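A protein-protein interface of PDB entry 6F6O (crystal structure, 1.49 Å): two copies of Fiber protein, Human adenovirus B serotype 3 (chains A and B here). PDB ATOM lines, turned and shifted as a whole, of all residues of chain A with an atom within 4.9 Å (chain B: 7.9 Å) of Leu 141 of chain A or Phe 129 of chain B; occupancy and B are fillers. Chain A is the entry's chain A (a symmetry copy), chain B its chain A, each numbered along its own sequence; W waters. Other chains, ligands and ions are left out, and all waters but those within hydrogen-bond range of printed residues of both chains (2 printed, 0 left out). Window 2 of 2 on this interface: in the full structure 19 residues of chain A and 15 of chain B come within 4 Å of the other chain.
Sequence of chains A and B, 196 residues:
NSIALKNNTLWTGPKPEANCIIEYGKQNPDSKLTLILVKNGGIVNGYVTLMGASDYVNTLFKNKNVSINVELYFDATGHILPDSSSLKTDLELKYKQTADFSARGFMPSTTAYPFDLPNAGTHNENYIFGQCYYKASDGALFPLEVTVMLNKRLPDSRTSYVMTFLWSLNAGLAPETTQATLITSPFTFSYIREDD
Leu 141 of chain A touches one residue of chain B. Phe 129 of chain B touches three residues of chain A. Ala 140 of chain A touches none of the printed residues of chain B. Of the printed residues of chain B, Lys 135 of chain A touches Asn 124 (3.9 Å). Printed residues of chain A within 4 Å of Asn 124 of chain B: Lys 135. Leu 166 of chain B touches none of the printed residues of chain A. The nearest residue of chain B that does not touch Leu 141 of chain A is Thr 147 of chain B (5.6 Å). The nearest printed residue of chain B that does not touch Tyr 133 of chain A is Gly 130 of chain B (4.1 Å).
Of the 17 printed residues of chain B, 3 touch a printed residue of chain A. Hydrophobic or aromatic side chains of chain B within 4 Å of the printed part of chain A: Phe 129. Of the 9 printed residues of chain A, 4 touch a printed residue of chain B. Printed residues of chain A that touch a printed residue of chain B: Tyr 133, Lys 135, Leu 141 and Ser 185. Among the printed residues, no Asp or Glu carboxylate lies within 4 Å of a Lys or Arg side-chain nitrogen of the other chain.
The backbone carbonyl oxygen (O) of Gly 139 of chain A lies within hydrogen-bond range of the side-chain amino group (NZ) of Lys 135 of chain A, at 2.9 Å. O of Tyr 133 of chain A lies within hydrogen-bond range of N of Ser 185 of chain A (2.9 Å).
No position is printed for both chains. Of the 5 pairs that touch across the chains among the printed residues, none has its exchanged pair printed and touching as well.
Water W2 lies within hydrogen-bond range of the backbone carbonyl oxygen of Lys 135 of chain A and the side-chain amide oxygen of Asn 124 of chain B. Water W1 bridges the side-chain hydroxyl of Ser 185 of chain A and the backbone carbonyl oxygen of Phe 129 of chain B.
CD1 of Tyr 133 of chain A touches CB of Phe 129 of chain B (3.4 Å). Lys 135 of chain A touches Asn 124 of chain B. Phe 129 of chain B touches Leu 141 of chain A (CZ to CD1, 3.6 Å). Ser 185 of chain A touches Tyr 127 of chain B. Ser 185 of chain A touches Phe 129 of chain B.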
ATOM      1  N   TYR A 133      -4.555  25.016 -13.546  1.00  0.00           N
ATOM      2  CA  TYR A 133      -4.550  26.358 -13.031  1.00  0.00           C
ATOM      3  C   TYR A 133      -5.649  27.223 -13.586  1.00  0.00           C
ATOM      4  O   TYR A 133      -6.147  26.951 -14.679  1.00  0.00           O
ATOM      5  CB  TYR A 133      -3.162  27.019 -13.311  1.00  0.00           C
ATOM      6  CG  TYR A 133      -1.957  26.213 -12.774  1.00  0.00           C
ATOM      7  CD1 TYR A 133      -1.503  25.084 -13.473  1.00  0.00           C
ATOM      8  CD2 TYR A 133      -1.398  26.521 -11.589  1.00  0.00           C
ATOM      9  CE1 TYR A 133      -0.473  24.284 -12.947  1.00  0.00           C
ATOM     10  CE2 TYR A 133      -0.344  25.765 -11.072  1.00  0.00           C
ATOM     11  CZ  TYR A 133       0.067  24.642 -11.758  1.00  0.00           C
ATOM     12  OH  TYR A 133       1.126  23.837 -11.292  1.00  0.00           O
ATOM     13  N   TYR A 134      -6.013  28.267 -12.843  1.00  0.00           N
ATOM     14  CA  TYR A 134      -6.937  29.323 -13.286  1.00  0.00           C
ATOM     15  C   TYR A 134      -6.222  30.648 -13.225  1.00  0.00           C
ATOM     16  O   TYR A 134      -5.658  30.966 -12.198  1.00  0.00           O
ATOM     17  CB  TYR A 134      -8.213  29.367 -12.434  1.00  0.00           C
ATOM     18  CG  TYR A 134      -9.141  30.501 -12.758  1.00  0.00           C
ATOM     19  CD1 TYR A 134      -9.896  30.523 -13.930  1.00  0.00           C
ATOM     20  CD2 TYR A 134      -9.247  31.607 -11.922  1.00  0.00           C
ATOM     21  CE1 TYR A 134     -10.693  31.612 -14.263  1.00  0.00           C
ATOM     22  CE2 TYR A 134     -10.060  32.669 -12.188  1.00  0.00           C
ATOM     23  CZ  TYR A 134     -10.834  32.659 -13.364  1.00  0.00           C
ATOM     24  OH  TYR A 134     -11.610  33.758 -13.679  1.00  0.00           O
ATOM     25  N   LYS A 135      -6.217  31.394 -14.335  1.00  0.00           N
ATOM     26  CA  LYS A 135      -5.633  32.693 -14.388  1.00  0.00           C
ATOM     27  C   LYS A 135      -6.738  33.701 -14.224  1.00  0.00           C
ATOM     28  O   LYS A 135      -7.636  33.838 -15.067  1.00  0.00           O
ATOM     29  CB  LYS A 135      -4.841  32.873 -15.709  1.00  0.00           C
ATOM     30  CG  LYS A 135      -4.158  34.246 -15.837  1.00  0.00           C
ATOM     31  CD  LYS A 135      -3.130  34.283 -16.977  1.00  0.00           C
ATOM     32  CE  LYS A 135      -2.395  35.621 -17.025  1.00  0.00           C
ATOM     33  NZ  LYS A 135      -1.339  35.641 -15.962  1.00  0.00           N
ATOM     34  N   GLY A 139      -4.585  38.824 -13.496  1.00  0.00           N
ATOM     35  CA  GLY A 139      -3.375  38.102 -13.863  1.00  0.00           C
ATOM     36  C   GLY A 139      -2.890  37.060 -12.872  1.00  0.00           C
ATOM     37  O   GLY A 139      -2.095  36.175 -13.223  1.00  0.00           O
ATOM     38  N   ALA A 140      -3.404  37.096 -11.652  1.00  0.00           N
ATOM     39  CA  ALA A 140      -2.950  36.154 -10.617  1.00  0.00           C
ATOM     40  C   ALA A 140      -3.338  34.694 -10.950  1.00  0.00           C
ATOM     41  O   ALA A 140      -4.451  34.387 -11.436  1.00  0.00           O
ATOM     42  CB  ALA A 140      -3.513  36.518  -9.255  1.00  0.00           C
ATOM     43  N   LEU A 141      -2.403  33.761 -10.715  1.00  0.00           N
ATOM     44  CA  LEU A 141      -2.590  32.364 -11.033  1.00  0.00           C
ATOM     45  C   LEU A 141      -2.970  31.554  -9.794  1.00  0.00           C
ATOM     46  O   LEU A 141      -2.396  31.765  -8.711  1.00  0.00           O
ATOM     47  CB  LEU A 141      -1.317  31.812 -11.700  1.00  0.00           C
ATOM     48  CG  LEU A 141      -1.381  30.492 -12.387  1.00  0.00           C
ATOM     49  CD1 LEU A 141      -2.176  30.584 -13.658  1.00  0.00           C
ATOM     50  CD2 LEU A 141       0.013  29.929 -12.683  1.00  0.00           C
ATOM     51  N   PHE A 142      -4.012  30.729  -9.909  1.00  0.00           N
ATOM     52  CA  PHE A 142      -4.478  29.880  -8.831  1.00  0.00           C
ATOM     53  C   PHE A 142      -4.370  28.400  -9.195  1.00  0.00           C
ATOM     54  O   PHE A 142      -4.848  28.002 -10.256  1.00  0.00           O
ATOM     55  CB  PHE A 142      -5.929  30.208  -8.474  1.00  0.00           C
ATOM     56  CG  PHE A 142      -6.116  31.548  -7.859  1.00  0.00           C
ATOM     57  CD1 PHE A 142      -6.215  32.690  -8.634  1.00  0.00           C
ATOM     58  CD2 PHE A 142      -6.111  31.708  -6.486  1.00  0.00           C
ATOM     59  CE1 PHE A 142      -6.318  33.964  -8.060  1.00  0.00           C
ATOM     60  CE2 PHE A 142      -6.275  32.958  -5.914  1.00  0.00           C
ATOM     61  CZ  PHE A 142      -6.341  34.089  -6.688  1.00  0.00           C
ATOM     62  N   PRO A 143      -3.800  27.577  -8.332  1.00  0.00           N
ATOM     63  CA  PRO A 143      -3.777  26.136  -8.616  1.00  0.00           C
ATOM     64  C   PRO A 143      -5.126  25.493  -8.348  1.00  0.00           C
ATOM     65  O   PRO A 143      -5.808  25.876  -7.365  1.00  0.00           O
ATOM     66  CB  PRO A 143      -2.735  25.583  -7.647  1.00  0.00           C
ATOM     67  CG  PRO A 143      -2.656  26.545  -6.564  1.00  0.00           C
ATOM     68  CD  PRO A 143      -3.131  27.920  -7.057  1.00  0.00           C
ATOM     69  N   SER A 185      -6.844  25.555 -17.140  1.00  0.00           N
ATOM     70  CA  SER A 185      -5.720  25.312 -18.075  1.00  0.00           C
ATOM     71  C   SER A 185      -5.653  23.825 -18.380  1.00  0.00           C
ATOM     72  O   SER A 185      -6.091  22.999 -17.564  1.00  0.00           O
ATOM     73  CB  SER A 185      -4.403  25.871 -17.485  1.00  0.00           C
ATOM     74  OG  SER A 185      -3.919  25.084 -16.419  1.00  0.00           O
ATOM     75  N   ASN B 124      -7.406  33.846 -22.968  1.00  0.00           N
ATOM     76  CA  ASN B 124      -6.668  33.208 -21.879  1.00  0.00           C
ATOM     77  C   ASN B 124      -6.611  31.663 -21.878  1.00  0.00           C
ATOM     78  O   ASN B 124      -5.835  31.050 -21.143  1.00  0.00           O
ATOM     79  CB  ASN B 124      -7.273  33.659 -20.546  1.00  0.00           C
ATOM     80  CG  ASN B 124      -6.524  34.762 -19.880  1.00  0.00           C
ATOM     81  OD1 ASN B 124      -6.813  35.038 -18.691  1.00  0.00           O
ATOM     82  ND2 ASN B 124      -5.645  35.443 -20.589  1.00  0.00           N
ATOM     83  N   GLU B 125      -7.259  31.064 -22.868  1.00  0.00           N
ATOM     84  CA  GLU B 125      -7.202  29.636 -23.051  1.00  0.00           C
ATOM     85  C   GLU B 125      -5.944  29.130 -23.750  1.00  0.00           C
ATOM     86  O   GLU B 125      -5.825  27.918 -24.056  1.00  0.00           O
ATOM     87  CB  GLU B 125      -8.451  29.110 -23.766  1.00  0.00           C
ATOM     88  CG  GLU B 125      -8.584  29.521 -25.218  1.00  0.00           C
ATOM     89  CD  GLU B 125      -9.361  30.795 -25.462  1.00  0.00           C
ATOM     90  OE1 GLU B 125      -9.364  31.730 -24.606  1.00  0.00           O
ATOM     91  OE2 GLU B 125     -10.021  30.888 -26.548  1.00  0.00           O
ATOM     92  N   ASN B 126      -4.982  30.017 -23.958  1.00  0.00           N
ATOM     93  CA  ASN B 126      -3.804  29.687 -24.738  1.00  0.00           C
ATOM     94  C   ASN B 126      -2.595  29.391 -23.887  1.00  0.00           C
ATOM     95  O   ASN B 126      -1.478  29.271 -24.416  1.00  0.00           O
ATOM     96  CB  ASN B 126      -3.492  30.880 -25.627  1.00  0.00           C
ATOM     97  CG  ASN B 126      -4.528  31.106 -26.730  1.00  0.00           C
ATOM     98  OD1 ASN B 126      -5.740  30.835 -26.579  1.00  0.00           O
ATOM     99  ND2 ASN B 126      -4.044  31.529 -27.887  1.00  0.00           N
ATOM    100  N   TYR B 127      -2.772  29.163 -22.583  1.00  0.00           N
ATOM    101  CA  TYR B 127      -1.680  28.908 -21.687  1.00  0.00           C
ATOM    102  C   TYR B 127      -1.686  27.487 -21.132  1.00  0.00           C
ATOM    103  O   TYR B 127      -2.745  26.994 -20.725  1.00  0.00           O
ATOM    104  CB  TYR B 127      -1.700  29.854 -20.482  1.00  0.00           C
ATOM    105  CG  TYR B 127      -1.491  31.326 -20.765  1.00  0.00           C
ATOM    106  CD1 TYR B 127      -0.257  31.813 -21.094  1.00  0.00           C
ATOM    107  CD2 TYR B 127      -2.570  32.215 -20.700  1.00  0.00           C
ATOM    108  CE1 TYR B 127      -0.047  33.186 -21.316  1.00  0.00           C
ATOM    109  CE2 TYR B 127      -2.369  33.570 -20.892  1.00  0.00           C
ATOM    110  CZ  TYR B 127      -1.098  34.030 -21.245  1.00  0.00           C
ATOM    111  OH  TYR B 127      -0.884  35.384 -21.457  1.00  0.00           O
ATOM    112  N   ILE B 128      -0.509  26.883 -21.026  1.00  0.00           N
ATOM    113  CA  ILE B 128      -0.311  25.650 -20.276  1.00  0.00           C
ATOM    114  C   ILE B 128       0.617  26.010 -19.136  1.00  0.00           C
ATOM    115  O   ILE B 128       1.643  26.673 -19.373  1.00  0.00           O
ATOM    116  CB  ILE B 128       0.364  24.580 -21.143  1.00  0.00           C
ATOM    117  CG1 ILE B 128      -0.608  24.190 -22.229  1.00  0.00           C
ATOM    118  CG2 ILE B 128       0.786  23.353 -20.336  1.00  0.00           C
ATOM    119  CD1 ILE B 128       0.019  23.456 -23.383  1.00  0.00           C
ATOM    120  N   PHE B 129       0.304  25.622 -17.933  1.00  0.00           N
ATOM    121  CA  PHE B 129       1.104  25.895 -16.771  1.00  0.00           C
ATOM    122  C   PHE B 129       1.514  24.603 -16.135  1.00  0.00           C
ATOM    123  O   PHE B 129       0.761  23.601 -16.142  1.00  0.00           O
ATOM    124  CB  PHE B 129       0.364  26.729 -15.733  1.00  0.00           C
ATOM    125  CG  PHE B 129      -0.252  27.999 -16.247  1.00  0.00           C
ATOM    126  CD1 PHE B 129       0.521  29.181 -16.340  1.00  0.00           C
ATOM    127  CD2 PHE B 129      -1.589  28.099 -16.589  1.00  0.00           C
ATOM    128  CE1 PHE B 129      -0.036  30.333 -16.789  1.00  0.00           C
ATOM    129  CE2 PHE B 129      -2.124  29.237 -17.033  1.00  0.00           C
ATOM    130  CZ  PHE B 129      -1.337  30.382 -17.184  1.00  0.00           C
ATOM    131  N   GLY B 130       2.702  24.582 -15.572  1.00  0.00           N
ATOM    132  CA  GLY B 130       3.171  23.464 -14.770  1.00  0.00           C
ATOM    133  C   GLY B 130       4.434  23.763 -14.022  1.00  0.00           C
ATOM    134  O   GLY B 130       4.719  24.933 -13.712  1.00  0.00           O
ATOM    135  N   GLN B 131       5.150  22.704 -13.614  1.00  0.00           N
ATOM    136  CA  GLN B 131       6.352  22.829 -12.827  1.00  0.00           C
ATOM    137  C   GLN B 131       7.418  21.908 -13.348  1.00  0.00           C
ATOM    138  O   GLN B 131       7.142  20.795 -13.828  1.00  0.00           O
ATOM    139  CB  GLN B 131       6.115  22.450 -11.361  1.00  0.00           C
ATOM    140  CG  GLN B 131       5.339  23.467 -10.571  1.00  0.00           C
ATOM    141  CD  GLN B 131       5.656  23.317  -9.089  1.00  0.00           C
ATOM    142  OE1 GLN B 131       5.632  24.268  -8.355  1.00  0.00           O
ATOM    143  NE2 GLN B 131       6.004  22.102  -8.675  1.00  0.00           N
ATOM    144  N   GLU B 145       8.380  27.384 -11.788  1.00  0.00           N
ATOM    145  CA  GLU B 145       7.079  27.506 -12.421  1.00  0.00           C
ATOM    146  C   GLU B 145       7.223  27.711 -13.906  1.00  0.00           C
ATOM    147  O   GLU B 145       8.037  28.552 -14.342  1.00  0.00           O
ATOM    148  CB  GLU B 145       6.341  28.710 -11.819  1.00  0.00           C
ATOM    149  CG  GLU B 145       6.273  28.766 -10.320  1.00  0.00           C
ATOM    150  CD  GLU B 145       5.825  27.487  -9.664  1.00  0.00           C
ATOM    151  OE1 GLU B 145       4.760  26.984 -10.113  1.00  0.00           O
ATOM    152  OE2 GLU B 145       6.501  27.005  -8.676  1.00  0.00           O
ATOM    153  N   VAL B 146       6.532  26.918 -14.697  1.00  0.00           N
ATOM    154  CA  VAL B 146       6.606  26.924 -16.153  1.00  0.00           C
ATOM    155  C   VAL B 146       5.299  27.437 -16.755  1.00  0.00           C
ATOM    156  O   VAL B 146       4.217  26.977 -16.396  1.00  0.00           O
ATOM    157  CB  VAL B 146       6.953  25.562 -16.812  1.00  0.00           C
ATOM    158  CG1 VAL B 146       7.075  25.692 -18.308  1.00  0.00           C
ATOM    159  CG2 VAL B 146       8.197  25.026 -16.236  1.00  0.00           C
ATOM    160  N   THR B 147       5.397  28.411 -17.682  1.00  0.00           N
ATOM    161  CA  THR B 147       4.275  28.810 -18.521  1.00  0.00           C
ATOM    162  C   THR B 147       4.613  28.636 -19.968  1.00  0.00           C
ATOM    163  O   THR B 147       5.643  29.140 -20.415  1.00  0.00           O
ATOM    164  CB  THR B 147       3.941  30.306 -18.277  1.00  0.00           C
ATOM    165  OG1 THR B 147       3.680  30.556 -16.910  1.00  0.00           O
ATOM    166  CG2 THR B 147       2.738  30.775 -19.105  1.00  0.00           C
ATOM    167  N   VAL B 148       3.767  27.943 -20.718  1.00  0.00           N
ATOM    168  CA  VAL B 148       3.841  27.832 -22.156  1.00  0.00           C
ATOM    169  C   VAL B 148       2.696  28.650 -22.690  1.00  0.00           C
ATOM    170  O   VAL B 148       1.539  28.481 -22.268  1.00  0.00           O
ATOM    171  CB  VAL B 148       3.707  26.393 -22.718  1.00  0.00           C
ATOM    172  CG1 VAL B 148       3.949  26.326 -24.194  1.00  0.00           C
ATOM    173  CG2 VAL B 148       4.691  25.450 -22.012  1.00  0.00           C
ATOM    174  N   MET B 149       2.991  29.608 -23.584  1.00  0.00           N
ATOM    175  CA  MET B 149       1.968  30.363 -24.309  1.00  0.00           C
ATOM    176  C   MET B 149       1.960  29.944 -25.756  1.00  0.00           C
ATOM    177  O   MET B 149       3.015  29.890 -26.410  1.00  0.00           O
ATOM    178  CB  MET B 149       2.192  31.856 -24.215  1.00  0.00           C
ATOM    179  CG  MET B 149       1.106  32.693 -24.865  1.00  0.00           C
ATOM    180  SD  MET B 149       1.467  34.471 -25.018  1.00  0.00           S
ATOM    181  CE  MET B 149       2.592  34.449 -26.401  1.00  0.00           C
ATOM    182  N   LEU B 166       8.323  30.281 -20.316  1.00  0.00           N
ATOM    183  CA  LEU B 166       8.818  31.039 -19.195  1.00  0.00           C
ATOM    184  C   LEU B 166       9.112  30.101 -18.041  1.00  0.00           C
ATOM    185  O   LEU B 166       8.208  29.325 -17.659  1.00  0.00           O
ATOM    186  CB  LEU B 166       7.818  32.111 -18.718  1.00  0.00           C
ATOM    187  CG  LEU B 166       8.098  32.790 -17.369  1.00  0.00           C
ATOM    188  CD1 LEU B 166       9.383  33.592 -17.399  1.00  0.00           C
ATOM    189  CD2 LEU B 166       6.953  33.710 -16.926  1.00  0.00           C
ATOM    190  N   PHE B 187      10.416  19.142 -18.989  1.00  0.00           N
ATOM    191  CA  PHE B 187       9.038  19.551 -18.835  1.00  0.00           C
ATOM    192  C   PHE B 187       8.260  18.987 -20.030  1.00  0.00           C
ATOM    193  O   PHE B 187       8.673  19.183 -21.161  1.00  0.00           O
ATOM    194  CB  PHE B 187       8.860  21.072 -18.756  1.00  0.00           C
ATOM    195  CG  PHE B 187       7.450  21.510 -18.596  1.00  0.00           C
ATOM    196  CD1 PHE B 187       6.748  21.232 -17.457  1.00  0.00           C
ATOM    197  CD2 PHE B 187       6.764  22.134 -19.662  1.00  0.00           C
ATOM    198  CE1 PHE B 187       5.413  21.577 -17.305  1.00  0.00           C
ATOM    199  CE2 PHE B 187       5.435  22.519 -19.474  1.00  0.00           C
ATOM    200  CZ  PHE B 187       4.749  22.182 -18.321  1.00  0.00           C
ATOM    201  N   THR B 188       7.174  18.304 -19.749  1.00  0.00           N
ATOM    202  CA  THR B 188       6.326  17.704 -20.779  1.00  0.00           C
ATOM    203  C   THR B 188       5.020  18.406 -20.803  1.00  0.00           C
ATOM    204  O   THR B 188       4.465  18.845 -19.759  1.00  0.00           O
ATOM    205  CB  THR B 188       6.157  16.221 -20.606  1.00  0.00           C
ATOM    206  OG1 THR B 188       5.616  15.952 -19.312  1.00  0.00           O
ATOM    207  CG2 THR B 188       7.462  15.470 -20.800  1.00  0.00           C
ATOM    208  N   PHE B 189       4.454  18.522 -22.025  1.00  0.00           N
ATOM    209  CA  PHE B 189       3.231  19.214 -22.257  1.00  0.00           C
ATOM    210  C   PHE B 189       2.605  18.686 -23.534  1.00  0.00           C
ATOM    211  O   PHE B 189       3.277  18.029 -24.320  1.00  0.00           O
ATOM    212  CB  PHE B 189       3.428  20.693 -22.322  1.00  0.00           C
ATOM    213  CG  PHE B 189       4.373  21.170 -23.414  1.00  0.00           C
ATOM    214  CD1 PHE B 189       5.754  21.051 -23.331  1.00  0.00           C
ATOM    215  CD2 PHE B 189       3.862  21.714 -24.560  1.00  0.00           C
ATOM    216  CE1 PHE B 189       6.595  21.510 -24.320  1.00  0.00           C
ATOM    217  CE2 PHE B 189       4.702  22.187 -25.543  1.00  0.00           C
ATOM    218  CZ  PHE B 189       6.061  22.038 -25.480  1.00  0.00           C
HETATM  219  O   HOH W   1      -2.008  23.484 -17.488  1.00  0.00           O
HETATM  220  O   HOH W   2      -8.402  32.725 -17.407  1.00  0.00           O
